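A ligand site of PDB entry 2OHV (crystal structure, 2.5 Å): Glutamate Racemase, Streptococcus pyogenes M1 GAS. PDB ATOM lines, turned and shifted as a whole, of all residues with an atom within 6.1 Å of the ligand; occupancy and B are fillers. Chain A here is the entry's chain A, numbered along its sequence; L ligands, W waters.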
ATOM      1  N   LEU A   9      -5.337  -5.696  12.006  1.00  0.00           N
ATOM      2  CA  LEU A   9      -5.144  -4.269  12.230  1.00  0.00           C
ATOM      3  C   LEU A   9      -4.786  -4.014  13.699  1.00  0.00           C
ATOM      4  O   LEU A   9      -5.622  -4.201  14.593  1.00  0.00           O
ATOM      5  CB  LEU A   9      -6.402  -3.487  11.828  1.00  0.00           C
ATOM      6  CG  LEU A   9      -7.657  -3.402  12.707  1.00  0.00           C
ATOM      7  CD1 LEU A   9      -7.465  -2.394  13.845  1.00  0.00           C
ATOM      8  CD2 LEU A   9      -8.796  -2.927  11.850  1.00  0.00           C
ATOM      9  N   ASP A  10      -3.551  -3.615  13.969  1.00  0.00           N
ATOM     10  CA  ASP A  10      -3.150  -3.330  15.343  1.00  0.00           C
ATOM     11  C   ASP A  10      -2.756  -1.863  15.495  1.00  0.00           C
ATOM     12  O   ASP A  10      -2.594  -1.141  14.513  1.00  0.00           O
ATOM     13  CB  ASP A  10      -1.978  -4.235  15.755  1.00  0.00           C
ATOM     14  CG  ASP A  10      -1.694  -4.155  17.249  1.00  0.00           C
ATOM     15  OD1 ASP A  10      -2.634  -4.371  18.041  1.00  0.00           O
ATOM     16  OD2 ASP A  10      -0.533  -3.882  17.624  1.00  0.00           O
ATOM     17  N   SER A  11      -2.599  -1.423  16.746  1.00  0.00           N
ATOM     18  CA  SER A  11      -2.234  -0.032  17.027  1.00  0.00           C
ATOM     19  C   SER A  11      -0.727   0.140  17.085  1.00  0.00           C
ATOM     20  O   SER A  11      -0.228   1.254  17.206  1.00  0.00           O
ATOM     21  CB  SER A  11      -2.860   0.412  18.348  1.00  0.00           C
ATOM     22  OG  SER A  11      -2.691  -0.552  19.371  1.00  0.00           O
ATOM     23  N   GLY A  12      -0.012  -0.964  16.990  1.00  0.00           N
ATOM     24  CA  GLY A  12       1.437  -0.922  17.059  1.00  0.00           C
ATOM     25  C   GLY A  12       1.963  -2.336  16.898  1.00  0.00           C
ATOM     26  O   GLY A  12       1.597  -3.045  15.968  1.00  0.00           O
ATOM     27  N   VAL A  13       2.807  -2.766  17.826  1.00  0.00           N
ATOM     28  CA  VAL A  13       3.397  -4.091  17.772  1.00  0.00           C
ATOM     29  C   VAL A  13       2.700  -5.092  18.713  1.00  0.00           C
ATOM     30  O   VAL A  13       2.995  -6.296  18.685  1.00  0.00           O
ATOM     31  CB  VAL A  13       4.894  -3.994  18.136  1.00  0.00           C
ATOM     32  CG1 VAL A  13       5.049  -3.706  19.622  1.00  0.00           C
ATOM     33  CG2 VAL A  13       5.611  -5.277  17.761  1.00  0.00           C
ATOM     34  N   GLY A  14       1.779  -4.612  19.531  1.00  0.00           N
ATOM     35  CA  GLY A  14       1.091  -5.482  20.463  1.00  0.00           C
ATOM     36  C   GLY A  14       0.367  -6.655  19.814  1.00  0.00           C
ATOM     37  O   GLY A  14       0.519  -7.815  20.228  1.00  0.00           O
ATOM     38  N   ASP A  36      -0.422   0.483  13.325  1.00  0.00           N
ATOM     39  CA  ASP A  36      -0.306   1.936  13.251  1.00  0.00           C
ATOM     40  C   ASP A  36       0.564   2.549  14.381  1.00  0.00           C
ATOM     41  O   ASP A  36       0.072   3.381  15.148  1.00  0.00           O
ATOM     42  CB  ASP A  36      -1.707   2.552  13.271  1.00  0.00           C
ATOM     43  CG  ASP A  36      -1.772   3.901  12.576  1.00  0.00           C
ATOM     44  OD1 ASP A  36      -0.710   4.396  12.144  1.00  0.00           O
ATOM     45  OD2 ASP A  36      -2.886   4.460  12.456  1.00  0.00           O
ATOM     46  N   ALA A  38       2.615   4.878  14.530  1.00  0.00           N
ATOM     47  CA  ALA A  38       2.485   6.334  14.569  1.00  0.00           C
ATOM     48  C   ALA A  38       1.047   6.679  14.904  1.00  0.00           C
ATOM     49  O   ALA A  38       0.173   5.811  14.827  1.00  0.00           O
ATOM     50  CB  ALA A  38       2.875   6.931  13.219  1.00  0.00           C
ATOM     51  N   ARG A  39       0.785   7.936  15.260  1.00  0.00           N
ATOM     52  CA  ARG A  39      -0.570   8.389  15.580  1.00  0.00           C
ATOM     53  C   ARG A  39      -1.038   7.966  16.983  1.00  0.00           C
ATOM     54  O   ARG A  39      -0.606   6.943  17.512  1.00  0.00           O
ATOM     55  CB  ARG A  39      -1.557   7.856  14.545  1.00  0.00           C
ATOM     56  CG  ARG A  39      -1.120   8.053  13.097  1.00  0.00           C
ATOM     57  CD  ARG A  39      -1.988   7.260  12.138  1.00  0.00           C
ATOM     58  NE  ARG A  39      -3.277   7.916  11.869  1.00  0.00           N
ATOM     59  CZ  ARG A  39      -4.297   7.316  11.275  1.00  0.00           C
ATOM     60  NH1 ARG A  39      -4.200   6.059  10.894  1.00  0.00           N
ATOM     61  NH2 ARG A  39      -5.418   7.995  11.056  1.00  0.00           N
ATOM     62  N   ALA A  40      -1.921   8.768  17.576  1.00  0.00           N
ATOM     63  CA  ALA A  40      -2.451   8.484  18.908  1.00  0.00           C
ATOM     64  C   ALA A  40      -3.661   9.360  19.218  1.00  0.00           C
ATOM     65  O   ALA A  40      -4.301   9.194  20.266  1.00  0.00           O
ATOM     66  CB  ALA A  40      -1.375   8.700  19.942  1.00  0.00           C
ATOM     67  N   ILE A  50     -10.454   7.758  17.001  1.00  0.00           N
ATOM     68  CA  ILE A  50      -9.926   6.411  16.935  1.00  0.00           C
ATOM     69  C   ILE A  50     -10.674   5.596  15.905  1.00  0.00           C
ATOM     70  O   ILE A  50     -10.082   4.729  15.249  1.00  0.00           O
ATOM     71  CB  ILE A  50      -9.967   5.715  18.334  1.00  0.00           C
ATOM     72  CG1 ILE A  50      -8.743   6.145  19.150  1.00  0.00           C
ATOM     73  CG2 ILE A  50     -10.021   4.186  18.198  1.00  0.00           C
ATOM     74  CD1 ILE A  50      -8.632   5.501  20.516  1.00  0.00           C
ATOM     75  N   TYR A  53      -9.266   6.423  12.562  1.00  0.00           N
ATOM     76  CA  TYR A  53      -7.978   5.764  12.413  1.00  0.00           C
ATOM     77  C   TYR A  53      -8.169   4.291  12.067  1.00  0.00           C
ATOM     78  O   TYR A  53      -7.521   3.766  11.168  1.00  0.00           O
ATOM     79  CB  TYR A  53      -7.175   5.878  13.709  1.00  0.00           C
ATOM     80  CG  TYR A  53      -6.503   7.215  13.943  1.00  0.00           C
ATOM     81  CD1 TYR A  53      -7.160   8.413  13.672  1.00  0.00           C
ATOM     82  CD2 TYR A  53      -5.223   7.278  14.483  1.00  0.00           C
ATOM     83  CE1 TYR A  53      -6.543   9.643  13.941  1.00  0.00           C
ATOM     84  CE2 TYR A  53      -4.608   8.492  14.746  1.00  0.00           C
ATOM     85  CZ  TYR A  53      -5.268   9.676  14.480  1.00  0.00           C
ATOM     86  OH  TYR A  53      -4.650  10.868  14.750  1.00  0.00           O
ATOM     87  N   THR A  54      -9.068   3.644  12.802  1.00  0.00           N
ATOM     88  CA  THR A  54      -9.330   2.230  12.577  1.00  0.00           C
ATOM     89  C   THR A  54      -9.804   2.017  11.152  1.00  0.00           C
ATOM     90  O   THR A  54      -9.289   1.154  10.446  1.00  0.00           O
ATOM     91  CB  THR A  54     -10.397   1.713  13.582  1.00  0.00           C
ATOM     92  OG1 THR A  54      -9.839   1.742  14.902  1.00  0.00           O
ATOM     93  CG2 THR A  54     -10.811   0.287  13.261  1.00  0.00           C
ATOM     94  N   LEU A  57      -7.194   1.899   8.641  1.00  0.00           N
ATOM     95  CA  LEU A  57      -6.482   0.619   8.653  1.00  0.00           C
ATOM     96  C   LEU A  57      -7.320  -0.506   8.067  1.00  0.00           C
ATOM     97  O   LEU A  57      -6.776  -1.476   7.538  1.00  0.00           O
ATOM     98  CB  LEU A  57      -6.079   0.258  10.078  1.00  0.00           C
ATOM     99  CG  LEU A  57      -5.156   1.223  10.825  1.00  0.00           C
ATOM    100  CD1 LEU A  57      -5.154   0.872  12.294  1.00  0.00           C
ATOM    101  CD2 LEU A  57      -3.766   1.162  10.268  1.00  0.00           C
ATOM    102  N   CYS A  73      -6.223  -5.139  18.327  1.00  0.00           N
ATOM    103  CA  CYS A  73      -6.117  -4.104  19.335  1.00  0.00           C
ATOM    104  C   CYS A  73      -7.386  -3.974  20.180  1.00  0.00           C
ATOM    105  O   CYS A  73      -8.482  -3.720  19.651  1.00  0.00           O
ATOM    106  CB  CYS A  73      -5.791  -2.770  18.693  1.00  0.00           C
ATOM    107  SG  CYS A  73      -5.820  -1.424  19.850  1.00  0.00           S
ATOM    108  N   ASN A  74      -7.213  -4.145  21.482  1.00  0.00           N
ATOM    109  CA  ASN A  74      -8.315  -4.078  22.434  1.00  0.00           C
ATOM    110  C   ASN A  74      -9.067  -2.746  22.398  1.00  0.00           C
ATOM    111  O   ASN A  74     -10.303  -2.708  22.464  1.00  0.00           O
ATOM    112  CB  ASN A  74      -7.794  -4.381  23.848  1.00  0.00           C
ATOM    113  CG  ASN A  74      -7.863  -5.873  24.205  1.00  0.00           C
ATOM    114  OD1 ASN A  74      -8.936  -6.407  24.482  1.00  0.00           O
ATOM    115  ND2 ASN A  74      -6.711  -6.555  24.193  1.00  0.00           N
ATOM    116  N   THR A  75      -8.322  -1.641  22.292  1.00  0.00           N
ATOM    117  CA  THR A  75      -8.932  -0.316  22.264  1.00  0.00           C
ATOM    118  C   THR A  75      -9.721  -0.098  20.980  1.00  0.00           C
ATOM    119  O   THR A  75     -10.880   0.344  21.014  1.00  0.00           O
ATOM    120  CB  THR A  75      -7.869   0.785  22.399  1.00  0.00           C
ATOM    121  OG1 THR A  75      -7.323   0.740  23.711  1.00  0.00           O
ATOM    122  CG2 THR A  75      -8.483   2.153  22.169  1.00  0.00           C
ATOM    123  N   ALA A  76      -9.090  -0.408  19.848  1.00  0.00           N
ATOM    124  CA  ALA A  76      -9.730  -0.289  18.548  1.00  0.00           C
ATOM    125  C   ALA A  76     -11.012  -1.142  18.554  1.00  0.00           C
ATOM    126  O   ALA A  76     -12.085  -0.703  18.125  1.00  0.00           O
ATOM    127  CB  ALA A  76      -8.769  -0.766  17.455  1.00  0.00           C
ATOM    128  N   THR A 117      -4.705  -1.736  28.991  1.00  0.00           N
ATOM    129  CA  THR A 117      -4.376  -0.358  28.681  1.00  0.00           C
ATOM    130  C   THR A 117      -5.345   0.657  29.305  1.00  0.00           C
ATOM    131  O   THR A 117      -6.502   0.337  29.572  1.00  0.00           O
ATOM    132  CB  THR A 117      -4.405  -0.210  27.150  1.00  0.00           C
ATOM    133  OG1 THR A 117      -3.056  -0.212  26.639  1.00  0.00           O
ATOM    134  CG2 THR A 117      -5.153   1.033  26.733  1.00  0.00           C
ATOM    135  N   PRO A 118      -4.858   1.879  29.571  1.00  0.00           N
ATOM    136  CA  PRO A 118      -5.671   2.960  30.159  1.00  0.00           C
ATOM    137  C   PRO A 118      -6.890   3.259  29.296  1.00  0.00           C
ATOM    138  O   PRO A 118      -8.007   3.484  29.813  1.00  0.00           O
ATOM    139  CB  PRO A 118      -4.701   4.135  30.212  1.00  0.00           C
ATOM    140  CG  PRO A 118      -3.397   3.446  30.553  1.00  0.00           C
ATOM    141  CD  PRO A 118      -3.421   2.225  29.620  1.00  0.00           C
ATOM    142  N   MET A 119      -6.688   3.270  27.987  1.00  0.00           N
ATOM    143  CA  MET A 119      -7.776   3.535  27.066  1.00  0.00           C
ATOM    144  C   MET A 119      -8.767   2.363  27.035  1.00  0.00           C
ATOM    145  O   MET A 119      -9.981   2.565  27.039  1.00  0.00           O
ATOM    146  CB  MET A 119      -7.236   3.791  25.649  1.00  0.00           C
ATOM    147  CG  MET A 119      -6.190   4.897  25.573  1.00  0.00           C
ATOM    148  SD  MET A 119      -5.906   5.515  23.896  1.00  0.00           S
ATOM    149  CE  MET A 119      -7.293   6.650  23.735  1.00  0.00           C
ATOM    150  N   THR A 120      -8.241   1.132  27.027  1.00  0.00           N
ATOM    151  CA  THR A 120      -9.129  -0.027  26.998  1.00  0.00           C
ATOM    152  C   THR A 120      -9.972  -0.014  28.261  1.00  0.00           C
ATOM    153  O   THR A 120     -11.189  -0.247  28.221  1.00  0.00           O
ATOM    154  CB  THR A 120      -8.370  -1.373  26.923  1.00  0.00           C
ATOM    155  OG1 THR A 120      -7.655  -1.457  25.697  1.00  0.00           O
ATOM    156  CG2 THR A 120      -9.341  -2.542  26.984  1.00  0.00           C
ATOM    157  N   VAL A 148       3.068  -2.189  28.977  1.00  0.00           N
ATOM    158  CA  VAL A 148       3.436  -2.097  27.563  1.00  0.00           C
ATOM    159  C   VAL A 148       4.898  -1.712  27.369  1.00  0.00           C
ATOM    160  O   VAL A 148       5.646  -2.396  26.641  1.00  0.00           O
ATOM    161  CB  VAL A 148       2.533  -1.079  26.802  1.00  0.00           C
ATOM    162  CG1 VAL A 148       3.153  -0.728  25.467  1.00  0.00           C
ATOM    163  CG2 VAL A 148       1.149  -1.674  26.587  1.00  0.00           C
ATOM    164  N   GLU A 152       7.946  -3.947  25.325  1.00  0.00           N
ATOM    165  CA  GLU A 152       8.688  -3.500  24.155  1.00  0.00           C
ATOM    166  C   GLU A 152      10.183  -3.419  24.420  1.00  0.00           C
ATOM    167  O   GLU A 152      10.988  -3.456  23.490  1.00  0.00           O
ATOM    168  CB  GLU A 152       8.153  -2.153  23.688  1.00  0.00           C
ATOM    169  CG  GLU A 152       6.641  -2.099  23.675  1.00  0.00           C
ATOM    170  CD  GLU A 152       6.102  -1.070  22.720  1.00  0.00           C
ATOM    171  OE1 GLU A 152       6.758  -0.028  22.532  1.00  0.00           O
ATOM    172  OE2 GLU A 152       5.010  -1.293  22.159  1.00  0.00           O
ATOM    173  N   CYS A 183      -4.888  -6.779  27.240  1.00  0.00           N
ATOM    174  CA  CYS A 183      -3.975  -6.060  26.357  1.00  0.00           C
ATOM    175  C   CYS A 183      -3.184  -7.150  25.658  1.00  0.00           C
ATOM    176  O   CYS A 183      -2.687  -8.078  26.312  1.00  0.00           O
ATOM    177  CB  CYS A 183      -3.039  -5.137  27.148  1.00  0.00           C
ATOM    178  SG  CYS A 183      -1.780  -4.294  26.162  1.00  0.00           S
ATOM    179  N   THR A 184      -3.053  -7.055  24.336  1.00  0.00           N
ATOM    180  CA  THR A 184      -2.337  -8.088  23.580  1.00  0.00           C
ATOM    181  C   THR A 184      -0.850  -8.093  23.882  1.00  0.00           C
ATOM    182  O   THR A 184      -0.121  -9.019  23.522  1.00  0.00           O
ATOM    183  CB  THR A 184      -2.613  -7.955  22.053  1.00  0.00           C
ATOM    184  OG1 THR A 184      -2.198  -6.677  21.571  1.00  0.00           O
ATOM    185  CG2 THR A 184      -4.090  -8.097  21.795  1.00  0.00           C
ATOM    186  N   HIS A 185      -0.390  -7.073  24.588  1.00  0.00           N
ATOM    187  CA  HIS A 185       1.008  -7.004  24.975  1.00  0.00           C
ATOM    188  C   HIS A 185       1.285  -7.949  26.145  1.00  0.00           C
ATOM    189  O   HIS A 185       2.318  -8.613  26.195  1.00  0.00           O
ATOM    190  CB  HIS A 185       1.367  -5.589  25.448  1.00  0.00           C
ATOM    191  CG  HIS A 185       1.900  -4.677  24.394  1.00  0.00           C
ATOM    192  ND1 HIS A 185       1.107  -3.801  23.693  1.00  0.00           N
ATOM    193  CD2 HIS A 185       3.172  -4.453  23.984  1.00  0.00           C
ATOM    194  CE1 HIS A 185       1.874  -3.048  22.910  1.00  0.00           C
ATOM    195  NE2 HIS A 185       3.126  -3.433  23.065  1.00  0.00           N
HETATM  196  C1  LIG L   1      -5.739   2.644  20.114  1.00  0.00           C
HETATM  197  C2  LIG L   1      -6.403   2.467  18.864  1.00  0.00           C
HETATM  198  C3  LIG L   1      -5.765   2.853  17.654  1.00  0.00           C
HETATM  199  C4  LIG L   1      -6.429   2.675  16.404  1.00  0.00           C
HETATM  200  C5  LIG L   1      -5.788   3.078  15.199  1.00  0.00           C
HETATM  201  C6  LIG L   1      -4.477   3.646  15.237  1.00  0.00           C
HETATM  202  C7  LIG L   1      -3.797   3.834  16.483  1.00  0.00           C
HETATM  203  C8  LIG L   1      -4.429   3.443  17.705  1.00  0.00           C
HETATM  204  C9  LIG L   1      -3.765   3.620  18.955  1.00  0.00           C
HETATM  205  C10 LIG L   1      -4.414   3.215  20.172  1.00  0.00           C
HETATM  206  C11 LIG L   1      -3.723   3.390  21.526  1.00  0.00           C
HETATM  207  C12 LIG L   1      -3.356   1.999  22.139  1.00  0.00           C
HETATM  208  C13 LIG L   1      -3.822   1.928  23.613  1.00  0.00           C
HETATM  209  O1  LIG L   1      -4.921   1.245  23.927  1.00  0.00           O
HETATM  210  O2  LIG L   1      -3.213   2.504  24.523  1.00  0.00           O
HETATM  211  C14 LIG L   1      -1.806   1.740  22.046  1.00  0.00           C
HETATM  212  C15 LIG L   1      -1.242   0.407  22.623  1.00  0.00           C
HETATM  213  N1  LIG L   1      -2.057  -0.745  22.108  1.00  0.00           N
HETATM  214  C16 LIG L   1       0.209   0.292  22.217  1.00  0.00           C
HETATM  215  O3  LIG L   1       1.077   0.965  22.742  1.00  0.00           O
HETATM  216  O4  LIG L   1       0.513  -0.570  21.246  1.00  0.00           O
HETATM  217  O   HOH W   1       0.067  -2.459  19.718  1.00  0.00           O
HETATM  218  O   HOH W   2      -4.663  -1.599  23.274  1.00  0.00           O
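N1 of the ligand is in hydrogen-bond range of OG of Ser 11, at 2.8 Å.
O2 of the ligand lies close to OG1 of Thr 117 (3.4 Å).
An oxygen (O1) of the ligand sits at hydrogen-bond distance from the side-chain hydroxyl (OG1) of Thr 75.
OG1 of Thr 75 lies within hydrogen-bond range of OG1 of Thr 120 (3.0 Å).
The backbone NH (N) of Thr 75 sits close to the side-chain sulfur (SG) of Cys 73.
The side-chain hydroxyl (OG) of Ser 11 lies within hydrogen-bond range of the side-chain sulfur (SG) of Cys 73.
The backbone NH (N) of Asp 36 sits at hydrogen-bond distance from the backbone carbonyl oxygen (O) of Asp 10, 3.0 Å away.
A ring nitrogen (NE2) of His 185 lies within hydrogen-bond range of the side-chain carboxylate of Glu 152 (3.0 Å).
The side-chain carboxylate (OD2) of Asp 36 lies within salt-bridge range of the guanidinium group (NH1) of Arg 39.
N of His 185 sits close to SG of Cys 183, at 3.5 Å.
The backbone carbonyl oxygen (O) of Ile 50 lies within hydrogen-bond range of the side-chain hydroxyl (OG1) of Thr 54 (3.0 Å).
Water W2 bridges O1 of the ligand (2.9 Å) and SG of Cys 73 (3.6 Å).
Merely in contact with the ligand: Asp 36, Tyr 53, Thr 54, Leu 57, Met 119, Val 148 and His 185.
Hydrophobic or aromatic side chains within 4 Å of the ligand: Tyr 53, Leu 57, Met 119, Val 148 and His 185.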
